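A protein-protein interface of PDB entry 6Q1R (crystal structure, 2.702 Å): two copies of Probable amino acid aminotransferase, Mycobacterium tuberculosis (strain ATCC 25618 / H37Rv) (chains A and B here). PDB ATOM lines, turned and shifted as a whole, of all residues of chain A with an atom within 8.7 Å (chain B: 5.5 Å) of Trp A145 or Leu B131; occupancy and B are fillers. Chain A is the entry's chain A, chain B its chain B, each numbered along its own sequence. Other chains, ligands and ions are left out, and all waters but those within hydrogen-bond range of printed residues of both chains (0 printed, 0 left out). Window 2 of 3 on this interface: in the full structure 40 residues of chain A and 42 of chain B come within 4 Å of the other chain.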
ATOM      1  N   LEU A  59      19.072   9.621 -38.331  1.00  0.00           N
ATOM      2  CA  LEU A  59      18.406  10.387 -37.290  1.00  0.00           C
ATOM      3  C   LEU A  59      18.232  11.849 -37.676  1.00  0.00           C
ATOM      4  O   LEU A  59      17.348  12.522 -37.138  1.00  0.00           O
ATOM      5  CB  LEU A  59      19.218  10.278 -36.003  1.00  0.00           C
ATOM      6  CG  LEU A  59      19.209   8.888 -35.372  1.00  0.00           C
ATOM      7  CD1 LEU A  59      20.121   8.845 -34.165  1.00  0.00           C
ATOM      8  CD2 LEU A  59      17.806   8.501 -34.989  1.00  0.00           C
ATOM      9  N   MET A  60      19.050  12.343 -38.606  1.00  0.00           N
ATOM     10  CA  MET A  60      19.056  13.740 -39.015  1.00  0.00           C
ATOM     11  C   MET A  60      18.372  13.969 -40.356  1.00  0.00           C
ATOM     12  O   MET A  60      18.397  15.096 -40.864  1.00  0.00           O
ATOM     13  CB  MET A  60      20.499  14.247 -39.079  1.00  0.00           C
ATOM     14  CG  MET A  60      21.123  14.469 -37.723  1.00  0.00           C
ATOM     15  SD  MET A  60      20.601  16.039 -37.026  1.00  0.00           S
ATOM     16  CE  MET A  60      21.573  17.190 -38.000  1.00  0.00           C
ATOM     17  N   LEU A 135      18.660  16.448 -18.997  1.00  0.00           N
ATOM     18  CA  LEU A 135      17.736  15.455 -19.510  1.00  0.00           C
ATOM     19  C   LEU A 135      17.590  14.299 -18.527  1.00  0.00           C
ATOM     20  O   LEU A 135      18.547  13.948 -17.825  1.00  0.00           O
ATOM     21  CB  LEU A 135      18.198  14.909 -20.863  1.00  0.00           C
ATOM     22  CG  LEU A 135      18.559  15.984 -21.885  1.00  0.00           C
ATOM     23  CD1 LEU A 135      19.292  15.371 -23.081  1.00  0.00           C
ATOM     24  CD2 LEU A 135      17.365  16.843 -22.288  1.00  0.00           C
ATOM     25  N   ASP A 138      15.313   8.391 -19.039  1.00  0.00           N
ATOM     26  CA  ASP A 138      14.376   7.942 -20.057  1.00  0.00           C
ATOM     27  C   ASP A 138      14.226   8.959 -21.191  1.00  0.00           C
ATOM     28  O   ASP A 138      13.268   8.887 -21.973  1.00  0.00           O
ATOM     29  CB  ASP A 138      13.025   7.594 -19.420  1.00  0.00           C
ATOM     30  CG  ASP A 138      12.393   8.764 -18.691  1.00  0.00           C
ATOM     31  OD1 ASP A 138      13.122   9.492 -17.983  1.00  0.00           O
ATOM     32  OD2 ASP A 138      11.174   8.980 -18.858  1.00  0.00           O
ATOM     33  N   GLY A 139      15.181   9.890 -21.287  1.00  0.00           N
ATOM     34  CA  GLY A 139      15.078  10.976 -22.247  1.00  0.00           C
ATOM     35  C   GLY A 139      15.273  10.556 -23.693  1.00  0.00           C
ATOM     36  O   GLY A 139      14.578  11.049 -24.587  1.00  0.00           O
ATOM     37  N   GLY A 140      16.225   9.657 -23.951  1.00  0.00           N
ATOM     38  CA  GLY A 140      16.539   9.309 -25.330  1.00  0.00           C
ATOM     39  C   GLY A 140      15.396   8.622 -26.056  1.00  0.00           C
ATOM     40  O   GLY A 140      15.181   8.855 -27.250  1.00  0.00           O
ATOM     41  N   ASP A 141      14.636   7.787 -25.352  1.00  0.00           N
ATOM     42  CA  ASP A 141      13.556   7.033 -25.979  1.00  0.00           C
ATOM     43  C   ASP A 141      12.226   7.775 -25.900  1.00  0.00           C
ATOM     44  O   ASP A 141      11.552   7.952 -26.920  1.00  0.00           O
ATOM     45  CB  ASP A 141      13.435   5.643 -25.348  1.00  0.00           C
ATOM     46  CG  ASP A 141      14.695   4.814 -25.523  1.00  0.00           C
ATOM     47  OD1 ASP A 141      15.378   4.970 -26.564  1.00  0.00           O
ATOM     48  OD2 ASP A 141      14.990   3.999 -24.624  1.00  0.00           O
ATOM     49  N   ALA A 142      11.836   8.214 -24.700  1.00  0.00           N
ATOM     50  CA  ALA A 142      10.560   8.901 -24.543  1.00  0.00           C
ATOM     51  C   ALA A 142      10.535  10.223 -25.299  1.00  0.00           C
ATOM     52  O   ALA A 142       9.452  10.765 -25.550  1.00  0.00           O
ATOM     53  CB  ALA A 142      10.263   9.137 -23.061  1.00  0.00           C
ATOM     54  N   MET A 143      11.701  10.745 -25.670  1.00  0.00           N
ATOM     55  CA  MET A 143      11.819  11.984 -26.437  1.00  0.00           C
ATOM     56  C   MET A 143      12.712  11.708 -27.643  1.00  0.00           C
ATOM     57  O   MET A 143      13.880  12.113 -27.685  1.00  0.00           O
ATOM     58  CB  MET A 143      12.357  13.121 -25.564  1.00  0.00           C
ATOM     59  CG  MET A 143      11.367  13.563 -24.480  1.00  0.00           C
ATOM     60  SD  MET A 143      12.017  14.692 -23.228  1.00  0.00           S
ATOM     61  CE  MET A 143      12.845  13.572 -22.118  1.00  0.00           C
ATOM     62  N   PRO A 144      12.178  11.010 -28.652  1.00  0.00           N
ATOM     63  CA  PRO A 144      12.985  10.711 -29.845  1.00  0.00           C
ATOM     64  C   PRO A 144      13.288  11.938 -30.680  1.00  0.00           C
ATOM     65  O   PRO A 144      14.297  11.953 -31.398  1.00  0.00           O
ATOM     66  CB  PRO A 144      12.117   9.704 -30.609  1.00  0.00           C
ATOM     67  CG  PRO A 144      10.723  10.041 -30.196  1.00  0.00           C
ATOM     68  CD  PRO A 144      10.804  10.487 -28.764  1.00  0.00           C
ATOM     69  N   TRP A 145      12.444  12.970 -30.605  1.00  0.00           N
ATOM     70  CA  TRP A 145      12.657  14.181 -31.387  1.00  0.00           C
ATOM     71  C   TRP A 145      13.934  14.915 -30.991  1.00  0.00           C
ATOM     72  O   TRP A 145      14.394  15.780 -31.745  1.00  0.00           O
ATOM     73  CB  TRP A 145      11.456  15.112 -31.234  1.00  0.00           C
ATOM     74  CG  TRP A 145      10.979  15.223 -29.819  1.00  0.00           C
ATOM     75  CD1 TRP A 145      11.455  16.066 -28.858  1.00  0.00           C
ATOM     76  CD2 TRP A 145       9.938  14.456 -29.201  1.00  0.00           C
ATOM     77  NE1 TRP A 145      10.772  15.877 -27.682  1.00  0.00           N
ATOM     78  CE2 TRP A 145       9.836  14.894 -27.865  1.00  0.00           C
ATOM     79  CE3 TRP A 145       9.082  13.444 -29.647  1.00  0.00           C
ATOM     80  CZ2 TRP A 145       8.914  14.354 -26.971  1.00  0.00           C
ATOM     81  CZ3 TRP A 145       8.166  12.908 -28.758  1.00  0.00           C
ATOM     82  CH2 TRP A 145       8.088  13.366 -27.435  1.00  0.00           C
ATOM     83  N   LEU A 146      14.524  14.588 -29.835  1.00  0.00           N
ATOM     84  CA  LEU A 146      15.715  15.273 -29.343  1.00  0.00           C
ATOM     85  C   LEU A 146      17.019  14.730 -29.915  1.00  0.00           C
ATOM     86  O   LEU A 146      18.081  15.265 -29.571  1.00  0.00           O
ATOM     87  CB  LEU A 146      15.771  15.210 -27.811  1.00  0.00           C
ATOM     88  CG  LEU A 146      14.642  15.912 -27.054  1.00  0.00           C
ATOM     89  CD1 LEU A 146      14.826  15.750 -25.556  1.00  0.00           C
ATOM     90  CD2 LEU A 146      14.570  17.390 -27.425  1.00  0.00           C
ATOM     91  N   ILE A 147      16.965  13.700 -30.768  1.00  0.00           N
ATOM     92  CA  ILE A 147      18.108  13.146 -31.504  1.00  0.00           C
ATOM     93  C   ILE A 147      19.374  13.067 -30.650  1.00  0.00           C
ATOM     94  O   ILE A 147      20.479  13.379 -31.112  1.00  0.00           O
ATOM     95  CB  ILE A 147      18.363  13.934 -32.811  1.00  0.00           C
ATOM     96  CG1 ILE A 147      18.782  15.388 -32.549  1.00  0.00           C
ATOM     97  CG2 ILE A 147      17.118  13.908 -33.686  1.00  0.00           C
ATOM     98  CD1 ILE A 147      19.095  16.179 -33.797  1.00  0.00           C
ATOM     99  N   ALA A 148      19.223  12.637 -29.398  1.00  0.00           N
ATOM    100  CA  ALA A 148      20.359  12.574 -28.488  1.00  0.00           C
ATOM    101  C   ALA A 148      21.401  11.552 -28.917  1.00  0.00           C
ATOM    102  O   ALA A 148      22.563  11.654 -28.502  1.00  0.00           O
ATOM    103  CB  ALA A 148      19.878  12.257 -27.074  1.00  0.00           C
ATOM    104  N   SER A 149      21.024  10.584 -29.746  1.00  0.00           N
ATOM    105  CA  SER A 149      21.913   9.501 -30.139  1.00  0.00           C
ATOM    106  C   SER A 149      22.779   9.835 -31.352  1.00  0.00           C
ATOM    107  O   SER A 149      23.519   8.964 -31.821  1.00  0.00           O
ATOM    108  CB  SER A 149      21.081   8.242 -30.423  1.00  0.00           C
ATOM    109  OG  SER A 149      21.875   7.068 -30.417  1.00  0.00           O
ATOM    110  N   ILE B 129       2.016  21.368 -31.940  1.00  0.00           N
ATOM    111  CA  ILE B 129       1.922  20.279 -30.975  1.00  0.00           C
ATOM    112  C   ILE B 129       2.788  20.609 -29.770  1.00  0.00           C
ATOM    113  O   ILE B 129       3.797  21.312 -29.876  1.00  0.00           O
ATOM    114  CB  ILE B 129       2.340  18.919 -31.576  1.00  0.00           C
ATOM    115  CG1 ILE B 129       3.778  18.980 -32.095  1.00  0.00           C
ATOM    116  CG2 ILE B 129       1.379  18.498 -32.666  1.00  0.00           C
ATOM    117  CD1 ILE B 129       4.300  17.651 -32.602  1.00  0.00           C
ATOM    118  N   THR B 130       2.375  20.108 -28.609  1.00  0.00           N
ATOM    119  CA  THR B 130       3.181  20.212 -27.403  1.00  0.00           C
ATOM    120  C   THR B 130       4.168  19.050 -27.337  1.00  0.00           C
ATOM    121  O   THR B 130       3.813  17.901 -27.617  1.00  0.00           O
ATOM    122  CB  THR B 130       2.301  20.214 -26.151  1.00  0.00           C
ATOM    123  OG1 THR B 130       1.504  19.024 -26.124  1.00  0.00           O
ATOM    124  CG2 THR B 130       1.396  21.436 -26.135  1.00  0.00           C
ATOM    125  N   LEU B 131       5.406  19.354 -26.955  1.00  0.00           N
ATOM    126  CA  LEU B 131       6.426  18.330 -26.793  1.00  0.00           C
ATOM    127  C   LEU B 131       7.195  18.581 -25.507  1.00  0.00           C
ATOM    128  O   LEU B 131       7.483  19.730 -25.163  1.00  0.00           O
ATOM    129  CB  LEU B 131       7.408  18.304 -27.974  1.00  0.00           C
ATOM    130  CG  LEU B 131       6.893  17.771 -29.310  1.00  0.00           C
ATOM    131  CD1 LEU B 131       7.987  17.822 -30.363  1.00  0.00           C
ATOM    132  CD2 LEU B 131       6.368  16.357 -29.142  1.00  0.00           C
ATOM    133  N   ASP B 132       7.535  17.500 -24.810  1.00  0.00           N
ATOM    134  CA  ASP B 132       8.347  17.606 -23.606  1.00  0.00           C
ATOM    135  C   ASP B 132       9.788  17.923 -23.995  1.00  0.00           C
ATOM    136  O   ASP B 132      10.429  17.146 -24.711  1.00  0.00           O
ATOM    137  CB  ASP B 132       8.269  16.306 -22.805  1.00  0.00           C
ATOM    138  CG  ASP B 132       8.795  16.454 -21.381  1.00  0.00           C
ATOM    139  OD1 ASP B 132       8.241  15.790 -20.476  1.00  0.00           O
ATOM    140  OD2 ASP B 132       9.729  17.255 -21.148  1.00  0.00           O
ATOM    141  N   ARG B 133      10.296  19.070 -23.531  1.00  0.00           N
ATOM    142  CA  ARG B 133      11.666  19.457 -23.856  1.00  0.00           C
ATOM    143  C   ARG B 133      12.678  18.599 -23.108  1.00  0.00           C
ATOM    144  O   ARG B 133      13.788  18.373 -23.603  1.00  0.00           O
ATOM    145  CB  ARG B 133      11.878  20.944 -23.544  1.00  0.00           C
ATOM    146  CG  ARG B 133      13.307  21.469 -23.724  1.00  0.00           C
ATOM    147  CD  ARG B 133      13.779  21.380 -25.170  1.00  0.00           C
ATOM    148  NE  ARG B 133      15.137  21.895 -25.348  1.00  0.00           N
ATOM    149  CZ  ARG B 133      16.245  21.190 -25.132  1.00  0.00           C
ATOM    150  NH1 ARG B 133      16.169  19.930 -24.722  1.00  0.00           N
ATOM    151  NH2 ARG B 133      17.431  21.746 -25.325  1.00  0.00           N
ATOM    152  N   VAL B 157      18.909  20.413 -33.046  1.00  0.00           N
ATOM    153  CA  VAL B 157      17.765  19.798 -32.377  1.00  0.00           C
ATOM    154  C   VAL B 157      16.498  20.590 -32.658  1.00  0.00           C
ATOM    155  O   VAL B 157      15.426  20.013 -32.872  1.00  0.00           O
ATOM    156  CB  VAL B 157      18.031  19.658 -30.866  1.00  0.00           C
ATOM    157  CG1 VAL B 157      16.761  19.260 -30.142  1.00  0.00           C
ATOM    158  CG2 VAL B 157      19.113  18.622 -30.613  1.00  0.00           C
ATOM    159  N   ALA B 160      15.413  19.482 -35.955  1.00  0.00           N
ATOM    160  CA  ALA B 160      14.897  18.121 -35.876  1.00  0.00           C
ATOM    161  C   ALA B 160      13.524  18.093 -35.215  1.00  0.00           C
ATOM    162  O   ALA B 160      12.660  17.292 -35.593  1.00  0.00           O
ATOM    163  CB  ALA B 160      15.878  17.232 -35.114  1.00  0.00           C
ATOM    164  N   VAL B 161      13.309  18.953 -34.216  1.00  0.00           N
ATOM    165  CA  VAL B 161      12.008  19.022 -33.561  1.00  0.00           C
ATOM    166  C   VAL B 161      10.951  19.481 -34.552  1.00  0.00           C
ATOM    167  O   VAL B 161       9.819  18.979 -34.557  1.00  0.00           O
ATOM    168  CB  VAL B 161      12.087  19.936 -32.326  1.00  0.00           C
ATOM    169  CG1 VAL B 161      10.722  20.491 -31.968  1.00  0.00           C
ATOM    170  CG2 VAL B 161      12.667  19.168 -31.157  1.00  0.00           C
ATOM    171  N   HIS B 164      10.179  16.633 -36.888  1.00  0.00           N
ATOM    172  CA  HIS B 164       9.294  15.700 -36.195  1.00  0.00           C
ATOM    173  C   HIS B 164       7.848  16.170 -36.254  1.00  0.00           C
ATOM    174  O   HIS B 164       6.939  15.385 -36.545  1.00  0.00           O
ATOM    175  CB  HIS B 164       9.748  15.543 -34.746  1.00  0.00           C
ATOM    176  CG  HIS B 164       8.824  14.722 -33.903  1.00  0.00           C
ATOM    177  ND1 HIS B 164       8.800  13.346 -33.951  1.00  0.00           N
ATOM    178  CD2 HIS B 164       7.898  15.083 -32.985  1.00  0.00           C
ATOM    179  CE1 HIS B 164       7.897  12.894 -33.098  1.00  0.00           C
ATOM    180  NE2 HIS B 164       7.336  13.928 -32.499  1.00  0.00           N
ATOM    181  N   VAL B 173       5.848  23.811 -32.767  1.00  0.00           N
ATOM    182  CA  VAL B 173       5.923  23.056 -31.521  1.00  0.00           C
ATOM    183  C   VAL B 173       5.909  24.028 -30.347  1.00  0.00           C
ATOM    184  O   VAL B 173       6.401  25.157 -30.446  1.00  0.00           O
ATOM    185  CB  VAL B 173       7.190  22.163 -31.474  1.00  0.00           C
ATOM    186  CG1 VAL B 173       7.306  21.431 -30.144  1.00  0.00           C
ATOM    187  CG2 VAL B 173       7.197  21.173 -32.615  1.00  0.00           C
ATOM    188  N   ILE B 174       5.324  23.592 -29.233  1.00  0.00           N
ATOM    189  CA  ILE B 174       5.410  24.300 -27.960  1.00  0.00           C
ATOM    190  C   ILE B 174       6.090  23.371 -26.960  1.00  0.00           C
ATOM    191  O   ILE B 174       5.529  22.331 -26.590  1.00  0.00           O
ATOM    192  CB  ILE B 174       4.030  24.743 -27.453  1.00  0.00           C
ATOM    193  CG1 ILE B 174       3.423  25.771 -28.411  1.00  0.00           C
ATOM    194  CG2 ILE B 174       4.131  25.303 -26.041  1.00  0.00           C
ATOM    195  CD1 ILE B 174       2.032  26.206 -28.027  1.00  0.00           C
ATOM    196  N   PHE B 175       7.301  23.734 -26.535  1.00  0.00           N
ATOM    197  CA  PHE B 175       8.028  22.941 -25.549  1.00  0.00           C
ATOM    198  C   PHE B 175       7.427  23.107 -24.156  1.00  0.00           C
ATOM    199  O   PHE B 175       7.054  24.210 -23.747  1.00  0.00           O
ATOM    200  CB  PHE B 175       9.504  23.341 -25.527  1.00  0.00           C
ATOM    201  CG  PHE B 175      10.325  22.684 -26.597  1.00  0.00           C
ATOM    202  CD1 PHE B 175      10.265  21.314 -26.787  1.00  0.00           C
ATOM    203  CD2 PHE B 175      11.138  23.434 -27.429  1.00  0.00           C
ATOM    204  CE1 PHE B 175      11.013  20.704 -27.773  1.00  0.00           C
ATOM    205  CE2 PHE B 175      11.887  22.827 -28.421  1.00  0.00           C
ATOM    206  CZ  PHE B 175      11.822  21.461 -28.591  1.00  0.00           C
ATOM    207  N   VAL B 176       7.345  22.000 -23.423  1.00  0.00           N
ATOM    208  CA  VAL B 176       6.839  21.991 -22.057  1.00  0.00           C
ATOM    209  C   VAL B 176       7.844  21.260 -21.173  1.00  0.00           C
ATOM    210  O   VAL B 176       8.399  20.229 -21.570  1.00  0.00           O
ATOM    211  CB  VAL B 176       5.437  21.346 -21.975  1.00  0.00           C
ATOM    212  CG1 VAL B 176       5.420  19.992 -22.672  1.00  0.00           C
ATOM    213  CG2 VAL B 176       4.976  21.223 -20.529  1.00  0.00           C
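The backbone carbonyl oxygen (O) of Asp B132 is in hydrogen-bond range of the indole nitrogen (NE1) of Trp A145, at 3.2 Å.
SD of Met A143 sits close to O of Asp B132, at 3.3 Å.
The backbone NH (N) of Arg B133 is in hydrogen-bond range of the backbone carbonyl oxygen (O) of Val B176, 3.0 Å away.
O of Ile B174 sits at hydrogen-bond distance from N of Leu B131.
The backbone carbonyl oxygen (O) of Leu B131 lies within hydrogen-bond range of the backbone NH (N) of Val B176 (2.9 Å).
Arg B133 touches Met A143.
CH2 of Trp A145 touches CD2 of Leu B131, at 3.8 Å.
Trp A145 touches Ala B160 (O to CB, 3.96 Å).
O of Trp A145 touches CG2 of Val B161, 3.8 Å away.
CE3 of Trp A145 touches NE2 of His B164, 3.4 Å away.
Arg B133 touches Leu A146 (O to CD1, 3.4 Å).
Leu A146 touches Val B157 (O to CG2, 3.7 Å).
Val B157 touches Ile A147 (CG2 to CG1, 3.8 Å).
Ile A147 touches Ala B160 (CD1 to CB, 3.6 Å).
Trp A145 touches five residues of chain B.
Printed residues of chain B within 4 Å of Ile A147: Val B157 and Ala B160.
Ser A149 touches none of the printed residues of chain B.
Leu B131 touches one residue of chain A.
Of the printed residues of chain A, Asp B132 touches Met A143 and Trp A145.
Of the printed residues of chain A, Arg B133 touches Met A143 (3.96 Å) and Leu A146 (3.4 Å).
Printed residues of chain A within 4 Å of Val B161: Trp A145 (3.8 Å).
The nearest residue of chain B that does not touch Trp A145 is Val B157 (4.5 Å).
The nearest residue of chain A that does not touch Leu B131 is Met A143 (6.6 Å).
Hydrophobic or aromatic side chains of chain A that line the printed part of chain B: Met A143, Trp A145, Leu A146 and Ile A147.
Along chain A the printed residues that touch a printed residue of chain B span positions 143 to 147.
Of the 13 printed residues of chain B, 7 touch a printed residue of chain A.
Printed residues of chain B that touch a printed residue of chain A: Leu B131, Asp B132, Arg B133, Val B157, Ala B160, Val B161 and His B164.
Among the printed residues, no Asp or Glu carboxylate lies within 4 Å of a Lys or Arg side-chain nitrogen of the other chain.
No position is printed for both chains.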
